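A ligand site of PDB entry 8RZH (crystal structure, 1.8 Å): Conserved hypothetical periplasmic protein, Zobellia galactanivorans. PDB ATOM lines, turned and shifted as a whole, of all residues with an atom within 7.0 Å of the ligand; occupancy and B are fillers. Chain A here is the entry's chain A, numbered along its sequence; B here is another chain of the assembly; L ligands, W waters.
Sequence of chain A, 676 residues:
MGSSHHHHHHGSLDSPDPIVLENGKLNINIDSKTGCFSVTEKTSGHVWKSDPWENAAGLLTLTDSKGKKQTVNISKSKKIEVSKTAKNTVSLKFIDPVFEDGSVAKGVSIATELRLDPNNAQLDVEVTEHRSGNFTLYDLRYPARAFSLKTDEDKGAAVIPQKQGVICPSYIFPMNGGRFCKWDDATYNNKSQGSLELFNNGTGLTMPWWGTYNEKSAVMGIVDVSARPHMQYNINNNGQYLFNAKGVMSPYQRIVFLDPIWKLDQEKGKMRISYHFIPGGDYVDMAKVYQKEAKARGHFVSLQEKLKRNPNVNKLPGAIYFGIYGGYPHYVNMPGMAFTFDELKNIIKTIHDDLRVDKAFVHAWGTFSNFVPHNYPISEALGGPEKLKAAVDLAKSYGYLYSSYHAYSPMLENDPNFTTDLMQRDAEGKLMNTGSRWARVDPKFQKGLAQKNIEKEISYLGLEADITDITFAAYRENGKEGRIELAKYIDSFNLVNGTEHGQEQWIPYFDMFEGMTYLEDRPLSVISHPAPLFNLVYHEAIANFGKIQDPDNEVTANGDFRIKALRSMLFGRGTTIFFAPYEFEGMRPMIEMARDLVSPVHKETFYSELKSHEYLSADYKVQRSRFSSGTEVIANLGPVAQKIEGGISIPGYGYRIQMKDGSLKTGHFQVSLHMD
The side-chain carboxylate (OD2) of Asp 185 of chain B lies within hydrogen-bond range of an oxygen (O3) of the ligand (2.7 Å).
NE2 of Gln 549 is in hydrogen-bond range of O1 of the ligand, 2.9 Å away.
The side-chain carboxylate (OD2) of Asp 469 lies within salt-bridge range of a nitrogen (N1) of the ligand.
An oxygen (O3) of the ligand sits at hydrogen-bond distance from a ring nitrogen (NE2) of His 330 (3.0 Å).
NE2 of His 330 sits at hydrogen-bond distance from OD1 of Asp 185 of chain B (3.2 Å).
The indole nitrogen (NE1) of Trp 438 is in hydrogen-bond range of the side-chain carboxylate (OD1) of Asp 185 of chain B (2.8 Å).
The side-chain amino group of Lys 547 lies within hydrogen-bond range of the side-chain amide oxygen of Gln 549 (2.8 Å).
A ring nitrogen (ND1) of His 330 is in hydrogen-bond range of the side-chain hydroxyl (OH) of Tyr 325, at 2.7 Å.
The backbone NH of Ile 548 lies within hydrogen-bond range of the side-chain carboxylate of Glu 514, 2.9 Å away.
N of Ile 470 lies within hydrogen-bond range of OE1 of Glu 500 (3.2 Å).
OE2 of Glu 500 is in salt-bridge range of NZ of Lys 547, 2.8 Å away.
NZ of Lys 547 is in salt-bridge range of OE2 of Glu 514 (2.8 Å).
Residues that only touch the ligand: Ile 548 (3.3 Å), Glu 500 (3.4 Å), Ile 470 (3.4 Å), Trp 365 (3.5 Å), Cys 181 of chain B (3.6 Å), Trp 438 (3.6 Å), Lys 547 (3.7 Å), Tyr 405 (3.8 Å) and Pro 329 (3.9 Å).
Hydrophobic or aromatic side chains that line the ligand: Pro 329, His 330, Trp 365, Trp 438, Ile 470 and Ile 548.
13 residues have an atom within 4 Å of the ligand: Pro 329, His 330, Trp 365, Tyr 405, Trp 438, Asp 469, Ile 470, Glu 500, Lys 547, Ile 548, Gln 549, Cys 181 of chain B and Asp 185 of chain B.
The nearest printed residue that does not touch the ligand is Glu 514 (5.0 Å).
Water W2 lies within hydrogen-bond range of O1 of the ligand (2.6 Å), OD1 of Asp 469 (2.7 Å), OE1 of Glu 514 (2.8 Å) and NZ of Lys 547 (3.5 Å).
Water W1 lies within hydrogen-bond range of OD2 of Asp 185 of chain B, NE2 of Gln 549, O of Cys 181 of chain B and O3 of the ligand.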
ATOM      1  N   TYR A 325     -21.997 -24.712  26.566  1.00  0.00           N
ATOM      2  CA  TYR A 325     -23.213 -24.435  25.821  1.00  0.00           C
ATOM      3  C   TYR A 325     -24.077 -23.439  26.581  1.00  0.00           C
ATOM      4  O   TYR A 325     -24.715 -23.798  27.589  1.00  0.00           O
ATOM      5  CB  TYR A 325     -23.983 -25.726  25.528  1.00  0.00           C
ATOM      6  CG  TYR A 325     -25.233 -25.349  24.773  1.00  0.00           C
ATOM      7  CD1 TYR A 325     -25.145 -24.981  23.414  1.00  0.00           C
ATOM      8  CD2 TYR A 325     -26.468 -25.310  25.410  1.00  0.00           C
ATOM      9  CE1 TYR A 325     -26.281 -24.604  22.731  1.00  0.00           C
ATOM     10  CE2 TYR A 325     -27.625 -24.929  24.731  1.00  0.00           C
ATOM     11  CZ  TYR A 325     -27.510 -24.568  23.397  1.00  0.00           C
ATOM     12  OH  TYR A 325     -28.623 -24.130  22.706  1.00  0.00           O
ATOM     13  N   TYR A 328     -27.029 -20.609  23.245  1.00  0.00           N
ATOM     14  CA  TYR A 328     -26.822 -19.968  21.943  1.00  0.00           C
ATOM     15  C   TYR A 328     -26.265 -21.010  20.996  1.00  0.00           C
ATOM     16  O   TYR A 328     -25.413 -21.792  21.408  1.00  0.00           O
ATOM     17  CB  TYR A 328     -25.839 -18.801  22.134  1.00  0.00           C
ATOM     18  CG  TYR A 328     -25.563 -17.917  20.949  1.00  0.00           C
ATOM     19  CD1 TYR A 328     -24.589 -18.268  20.003  1.00  0.00           C
ATOM     20  CD2 TYR A 328     -26.211 -16.687  20.810  1.00  0.00           C
ATOM     21  CE1 TYR A 328     -24.325 -17.420  18.912  1.00  0.00           C
ATOM     22  CE2 TYR A 328     -25.933 -15.830  19.734  1.00  0.00           C
ATOM     23  CZ  TYR A 328     -25.001 -16.215  18.792  1.00  0.00           C
ATOM     24  OH  TYR A 328     -24.761 -15.378  17.734  1.00  0.00           O
ATOM     25  N   PRO A 329     -26.684 -21.058  19.708  1.00  0.00           N
ATOM     26  CA  PRO A 329     -27.381 -20.000  18.930  1.00  0.00           C
ATOM     27  C   PRO A 329     -28.899 -19.974  19.059  1.00  0.00           C
ATOM     28  O   PRO A 329     -29.556 -19.088  18.510  1.00  0.00           O
ATOM     29  CB  PRO A 329     -26.987 -20.340  17.472  1.00  0.00           C
ATOM     30  CG  PRO A 329     -26.882 -21.859  17.478  1.00  0.00           C
ATOM     31  CD  PRO A 329     -26.226 -22.169  18.859  1.00  0.00           C
ATOM     32  N   HIS A 330     -29.448 -20.928  19.841  1.00  0.00           N
ATOM     33  CA  HIS A 330     -30.902 -21.042  19.950  1.00  0.00           C
ATOM     34  C   HIS A 330     -31.540 -19.804  20.562  1.00  0.00           C
ATOM     35  O   HIS A 330     -32.638 -19.420  20.169  1.00  0.00           O
ATOM     36  CB  HIS A 330     -31.207 -22.291  20.781  1.00  0.00           C
ATOM     37  CG  HIS A 330     -30.663 -23.517  20.149  1.00  0.00           C
ATOM     38  ND1 HIS A 330     -29.309 -23.801  20.077  1.00  0.00           N
ATOM     39  CD2 HIS A 330     -31.308 -24.491  19.448  1.00  0.00           C
ATOM     40  CE1 HIS A 330     -29.146 -24.904  19.367  1.00  0.00           C
ATOM     41  NE2 HIS A 330     -30.335 -25.350  18.987  1.00  0.00           N
ATOM     42  N   TRP A 365     -20.196 -21.446  23.225  1.00  0.00           N
ATOM     43  CA  TRP A 365     -21.446 -21.207  22.499  1.00  0.00           C
ATOM     44  C   TRP A 365     -22.231 -20.124  23.207  1.00  0.00           C
ATOM     45  O   TRP A 365     -22.978 -20.382  24.160  1.00  0.00           O
ATOM     46  CB  TRP A 365     -22.277 -22.484  22.412  1.00  0.00           C
ATOM     47  CG  TRP A 365     -21.640 -23.614  21.673  1.00  0.00           C
ATOM     48  CD1 TRP A 365     -20.341 -24.039  21.752  1.00  0.00           C
ATOM     49  CD2 TRP A 365     -22.296 -24.505  20.759  1.00  0.00           C
ATOM     50  NE1 TRP A 365     -20.148 -25.141  20.932  1.00  0.00           N
ATOM     51  CE2 TRP A 365     -21.332 -25.424  20.286  1.00  0.00           C
ATOM     52  CE3 TRP A 365     -23.605 -24.560  20.242  1.00  0.00           C
ATOM     53  CZ2 TRP A 365     -21.637 -26.412  19.366  1.00  0.00           C
ATOM     54  CZ3 TRP A 365     -23.900 -25.554  19.309  1.00  0.00           C
ATOM     55  CH2 TRP A 365     -22.929 -26.468  18.887  1.00  0.00           C
ATOM     56  N   TYR A 405     -18.804 -19.983  19.039  1.00  0.00           N
ATOM     57  CA  TYR A 405     -19.746 -20.620  18.117  1.00  0.00           C
ATOM     58  C   TYR A 405     -19.989 -19.670  16.939  1.00  0.00           C
ATOM     59  O   TYR A 405     -20.300 -18.501  17.147  1.00  0.00           O
ATOM     60  CB  TYR A 405     -21.077 -20.965  18.820  1.00  0.00           C
ATOM     61  CG  TYR A 405     -22.103 -21.547  17.819  1.00  0.00           C
ATOM     62  CD1 TYR A 405     -22.912 -20.711  17.045  1.00  0.00           C
ATOM     63  CD2 TYR A 405     -22.181 -22.921  17.600  1.00  0.00           C
ATOM     64  CE1 TYR A 405     -23.806 -21.229  16.093  1.00  0.00           C
ATOM     65  CE2 TYR A 405     -23.070 -23.443  16.678  1.00  0.00           C
ATOM     66  CZ  TYR A 405     -23.881 -22.582  15.924  1.00  0.00           C
ATOM     67  OH  TYR A 405     -24.766 -23.097  14.995  1.00  0.00           O
ATOM     68  N   ALA A 407     -22.010 -19.519  12.889  1.00  0.00           N
ATOM     69  CA  ALA A 407     -22.764 -20.170  11.828  1.00  0.00           C
ATOM     70  C   ALA A 407     -23.257 -19.116  10.840  1.00  0.00           C
ATOM     71  O   ALA A 407     -23.685 -18.040  11.245  1.00  0.00           O
ATOM     72  CB  ALA A 407     -23.952 -20.962  12.403  1.00  0.00           C
ATOM     73  N   PRO A 410     -27.972 -20.308   9.307  1.00  0.00           N
ATOM     74  CA  PRO A 410     -29.340 -20.282   9.863  1.00  0.00           C
ATOM     75  C   PRO A 410     -30.112 -19.044   9.450  1.00  0.00           C
ATOM     76  O   PRO A 410     -29.565 -18.000   9.134  1.00  0.00           O
ATOM     77  CB  PRO A 410     -29.120 -20.291  11.399  1.00  0.00           C
ATOM     78  CG  PRO A 410     -27.760 -20.912  11.568  1.00  0.00           C
ATOM     79  CD  PRO A 410     -26.973 -20.334  10.389  1.00  0.00           C
ATOM     80  N   TRP A 438     -31.826 -24.277  10.584  1.00  0.00           N
ATOM     81  CA  TRP A 438     -30.382 -24.073  10.704  1.00  0.00           C
ATOM     82  C   TRP A 438     -29.680 -24.010   9.356  1.00  0.00           C
ATOM     83  O   TRP A 438     -28.516 -23.632   9.301  1.00  0.00           O
ATOM     84  CB  TRP A 438     -29.746 -25.171  11.584  1.00  0.00           C
ATOM     85  CG  TRP A 438     -30.327 -25.059  12.994  1.00  0.00           C
ATOM     86  CD1 TRP A 438     -31.247 -25.902  13.593  1.00  0.00           C
ATOM     87  CD2 TRP A 438     -30.099 -23.980  13.914  1.00  0.00           C
ATOM     88  NE1 TRP A 438     -31.588 -25.403  14.842  1.00  0.00           N
ATOM     89  CE2 TRP A 438     -30.882 -24.245  15.069  1.00  0.00           C
ATOM     90  CE3 TRP A 438     -29.267 -22.855  13.902  1.00  0.00           C
ATOM     91  CZ2 TRP A 438     -30.880 -23.392  16.193  1.00  0.00           C
ATOM     92  CZ3 TRP A 438     -29.270 -21.992  15.017  1.00  0.00           C
ATOM     93  CH2 TRP A 438     -30.086 -22.262  16.147  1.00  0.00           C
ATOM     94  N   ASP A 469     -20.275 -23.999  12.252  1.00  0.00           N
ATOM     95  CA  ASP A 469     -21.350 -24.984  12.389  1.00  0.00           C
ATOM     96  C   ASP A 469     -22.063 -25.184  11.050  1.00  0.00           C
ATOM     97  O   ASP A 469     -22.070 -24.295  10.200  1.00  0.00           O
ATOM     98  CB  ASP A 469     -22.371 -24.503  13.429  1.00  0.00           C
ATOM     99  CG  ASP A 469     -23.083 -25.648  14.136  1.00  0.00           C
ATOM    100  OD1 ASP A 469     -22.507 -26.741  14.258  1.00  0.00           O
ATOM    101  OD2 ASP A 469     -24.220 -25.425  14.582  1.00  0.00           O
ATOM    102  N   ILE A 470     -22.694 -26.368  10.906  1.00  0.00           N
ATOM    103  CA  ILE A 470     -23.787 -26.713   9.990  1.00  0.00           C
ATOM    104  C   ILE A 470     -23.348 -26.867   8.527  1.00  0.00           C
ATOM    105  O   ILE A 470     -23.660 -27.888   7.894  1.00  0.00           O
ATOM    106  CB  ILE A 470     -24.960 -25.714  10.095  1.00  0.00           C
ATOM    107  CG1 ILE A 470     -25.588 -25.730  11.500  1.00  0.00           C
ATOM    108  CG2 ILE A 470     -26.029 -26.014   9.044  1.00  0.00           C
ATOM    109  CD1 ILE A 470     -26.126 -24.286  11.913  1.00  0.00           C
ATOM    110  N   GLU A 500     -18.789 -28.881  12.062  1.00  0.00           N
ATOM    111  CA  GLU A 500     -19.723 -29.900  12.505  1.00  0.00           C
ATOM    112  C   GLU A 500     -19.770 -31.053  11.492  1.00  0.00           C
ATOM    113  O   GLU A 500     -20.065 -30.824  10.313  1.00  0.00           O
ATOM    114  CB  GLU A 500     -21.127 -29.308  12.646  1.00  0.00           C
ATOM    115  CG  GLU A 500     -22.114 -30.433  12.980  1.00  0.00           C
ATOM    116  CD  GLU A 500     -23.588 -30.032  12.902  1.00  0.00           C
ATOM    117  OE1 GLU A 500     -23.909 -29.006  12.259  1.00  0.00           O
ATOM    118  OE2 GLU A 500     -24.438 -30.776  13.482  1.00  0.00           O
ATOM    119  N   GLU A 514     -16.218 -32.308  14.282  1.00  0.00           N
ATOM    120  CA  GLU A 514     -16.995 -32.586  15.503  1.00  0.00           C
ATOM    121  C   GLU A 514     -18.149 -33.502  15.083  1.00  0.00           C
ATOM    122  O   GLU A 514     -19.141 -33.052  14.479  1.00  0.00           O
ATOM    123  CB  GLU A 514     -17.513 -31.277  16.120  1.00  0.00           C
ATOM    124  CG  GLU A 514     -18.623 -31.459  17.228  1.00  0.00           C
ATOM    125  CD  GLU A 514     -20.044 -31.201  16.686  1.00  0.00           C
ATOM    126  OE1 GLU A 514     -20.215 -30.223  15.880  1.00  0.00           O
ATOM    127  OE2 GLU A 514     -20.987 -31.923  17.053  1.00  0.00           O
ATOM    128  N   LYS A 547     -19.742 -36.099  18.856  1.00  0.00           N
ATOM    129  CA  LYS A 547     -20.768 -35.141  18.483  1.00  0.00           C
ATOM    130  C   LYS A 547     -21.356 -34.425  19.716  1.00  0.00           C
ATOM    131  O   LYS A 547     -21.591 -35.047  20.756  1.00  0.00           O
ATOM    132  CB  LYS A 547     -21.922 -35.892  17.768  1.00  0.00           C
ATOM    133  CG  LYS A 547     -22.935 -34.968  17.056  1.00  0.00           C
ATOM    134  CD  LYS A 547     -22.336 -34.565  15.654  1.00  0.00           C
ATOM    135  CE  LYS A 547     -23.231 -33.513  14.936  1.00  0.00           C
ATOM    136  NZ  LYS A 547     -23.395 -32.208  15.698  1.00  0.00           N
ATOM    137  N   ILE A 548     -21.643 -33.127  19.570  1.00  0.00           N
ATOM    138  CA  ILE A 548     -22.111 -32.379  20.746  1.00  0.00           C
ATOM    139  C   ILE A 548     -23.481 -32.860  21.223  1.00  0.00           C
ATOM    140  O   ILE A 548     -23.766 -32.778  22.417  1.00  0.00           O
ATOM    141  CB  ILE A 548     -22.124 -30.843  20.508  1.00  0.00           C
ATOM    142  CG1 ILE A 548     -23.054 -30.419  19.356  1.00  0.00           C
ATOM    143  CG2 ILE A 548     -20.689 -30.344  20.189  1.00  0.00           C
ATOM    144  CD1 ILE A 548     -24.445 -29.927  19.869  1.00  0.00           C
ATOM    145  N   GLN A 549     -24.347 -33.371  20.339  1.00  0.00           N
ATOM    146  CA  GLN A 549     -25.641 -33.885  20.806  1.00  0.00           C
ATOM    147  C   GLN A 549     -25.497 -35.155  21.639  1.00  0.00           C
ATOM    148  O   GLN A 549     -26.410 -35.472  22.423  1.00  0.00           O
ATOM    149  CB  GLN A 549     -26.568 -34.212  19.632  1.00  0.00           C
ATOM    150  CG  GLN A 549     -27.243 -32.975  18.975  1.00  0.00           C
ATOM    151  CD  GLN A 549     -26.376 -32.234  17.997  1.00  0.00           C
ATOM    152  OE1 GLN A 549     -25.197 -32.589  17.770  1.00  0.00           O
ATOM    153  NE2 GLN A 549     -26.954 -31.164  17.376  1.00  0.00           N
ATOM    154  N   PHE A 578     -19.510 -31.819  26.567  1.00  0.00           N
ATOM    155  CA  PHE A 578     -20.405 -30.778  26.099  1.00  0.00           C
ATOM    156  C   PHE A 578     -21.477 -30.552  27.154  1.00  0.00           C
ATOM    157  O   PHE A 578     -22.275 -31.457  27.429  1.00  0.00           O
ATOM    158  CB  PHE A 578     -21.087 -31.165  24.782  1.00  0.00           C
ATOM    159  CG  PHE A 578     -21.715 -30.002  24.078  1.00  0.00           C
ATOM    160  CD1 PHE A 578     -20.930 -29.116  23.388  1.00  0.00           C
ATOM    161  CD2 PHE A 578     -23.115 -29.813  24.099  1.00  0.00           C
ATOM    162  CE1 PHE A 578     -21.506 -27.997  22.707  1.00  0.00           C
ATOM    163  CE2 PHE A 578     -23.694 -28.725  23.406  1.00  0.00           C
ATOM    164  CZ  PHE A 578     -22.890 -27.825  22.724  1.00  0.00           C
ATOM    165  N   PHE B 180     -30.455 -29.995  25.060  1.00  0.00           N
ATOM    166  CA  PHE B 180     -31.119 -28.714  24.766  1.00  0.00           C
ATOM    167  C   PHE B 180     -31.219 -28.498  23.263  1.00  0.00           C
ATOM    168  O   PHE B 180     -32.285 -28.137  22.739  1.00  0.00           O
ATOM    169  CB  PHE B 180     -30.294 -27.571  25.431  1.00  0.00           C
ATOM    170  CG  PHE B 180     -30.982 -26.208  25.422  1.00  0.00           C
ATOM    171  CD1 PHE B 180     -31.039 -25.465  24.244  1.00  0.00           C
ATOM    172  CD2 PHE B 180     -31.503 -25.665  26.580  1.00  0.00           C
ATOM    173  CE1 PHE B 180     -31.659 -24.211  24.229  1.00  0.00           C
ATOM    174  CE2 PHE B 180     -32.107 -24.397  26.588  1.00  0.00           C
ATOM    175  CZ  PHE B 180     -32.185 -23.674  25.394  1.00  0.00           C
ATOM    176  N   CYS B 181     -30.107 -28.679  22.546  1.00  0.00           N
ATOM    177  CA  CYS B 181     -30.109 -28.542  21.096  1.00  0.00           C
ATOM    178  C   CYS B 181     -31.144 -29.472  20.463  1.00  0.00           C
ATOM    179  O   CYS B 181     -31.930 -29.034  19.615  1.00  0.00           O
ATOM    180  CB  CYS B 181     -28.719 -28.862  20.538  1.00  0.00           C
ATOM    181  SG  CYS B 181     -27.506 -27.550  20.951  1.00  0.00           S
ATOM    182  N   LYS B 182     -31.174 -30.762  20.881  1.00  0.00           N
ATOM    183  CA  LYS B 182     -32.153 -31.683  20.291  1.00  0.00           C
ATOM    184  C   LYS B 182     -33.577 -31.292  20.655  1.00  0.00           C
ATOM    185  O   LYS B 182     -34.517 -31.473  19.857  1.00  0.00           O
ATOM    186  CB  LYS B 182     -31.883 -33.122  20.771  1.00  0.00           C
ATOM    187  CG  LYS B 182     -30.579 -33.684  20.130  1.00  0.00           C
ATOM    188  CD  LYS B 182     -30.383 -35.195  20.533  1.00  0.00           C
ATOM    189  CE  LYS B 182     -29.861 -35.246  21.989  1.00  0.00           C
ATOM    190  NZ  LYS B 182     -29.732 -36.696  22.444  1.00  0.00           N
ATOM    191  N   ASP B 184     -34.899 -28.207  21.610  1.00  0.00           N
ATOM    192  CA  ASP B 184     -35.381 -26.996  20.951  1.00  0.00           C
ATOM    193  C   ASP B 184     -35.595 -27.234  19.458  1.00  0.00           C
ATOM    194  O   ASP B 184     -36.593 -26.789  18.874  1.00  0.00           O
ATOM    195  CB  ASP B 184     -34.380 -25.854  21.160  1.00  0.00           C
ATOM    196  CG  ASP B 184     -35.022 -24.473  20.934  1.00  0.00           C
ATOM    197  OD1 ASP B 184     -35.948 -24.145  21.717  1.00  0.00           O
ATOM    198  OD2 ASP B 184     -34.602 -23.737  19.991  1.00  0.00           O
ATOM    199  N   ASP B 185     -34.647 -27.939  18.821  1.00  0.00           N
ATOM    200  CA  ASP B 185     -34.753 -28.197  17.379  1.00  0.00           C
ATOM    201  C   ASP B 185     -36.016 -28.974  17.036  1.00  0.00           C
ATOM    202  O   ASP B 185     -36.660 -28.708  16.002  1.00  0.00           O
ATOM    203  CB  ASP B 185     -33.550 -28.980  16.894  1.00  0.00           C
ATOM    204  CG  ASP B 185     -32.310 -28.120  16.800  1.00  0.00           C
ATOM    205  OD1 ASP B 185     -32.394 -26.908  17.114  1.00  0.00           O
ATOM    206  OD2 ASP B 185     -31.252 -28.655  16.418  1.00  0.00           O
HETATM  207  C1  LIG L   1     -25.805 -27.857  14.790  1.00  0.00           C
HETATM  208  C2  LIG L   1     -25.563 -27.781  16.410  1.00  0.00           C
HETATM  209  C3  LIG L   1     -26.768 -27.405  17.161  1.00  0.00           C
HETATM  210  C4  LIG L   1     -27.908 -27.606  16.452  1.00  0.00           C
HETATM  211  C5  LIG L   1     -28.011 -26.734  15.426  1.00  0.00           C
HETATM  212  C6  LIG L   1     -27.586 -25.445  16.066  1.00  0.00           C
HETATM  213  N1  LIG L   1     -27.056 -26.993  14.343  1.00  0.00           N
HETATM  214  O1  LIG L   1     -25.105 -29.079  16.707  1.00  0.00           O
HETATM  215  O2  LIG L   1     -26.756 -25.904  17.285  1.00  0.00           O
HETATM  216  O3  LIG L   1     -29.046 -27.461  17.281  1.00  0.00           O
HETATM  217  O   HOH W   1     -29.815 -30.828  17.591  1.00  0.00           O
HETATM  218  O   HOH W   2     -22.606 -28.861  15.978  1.00  0.00           O
HETATM  219  O   HOH W   3     -28.379 -28.294  12.508  1.00  0.00           O
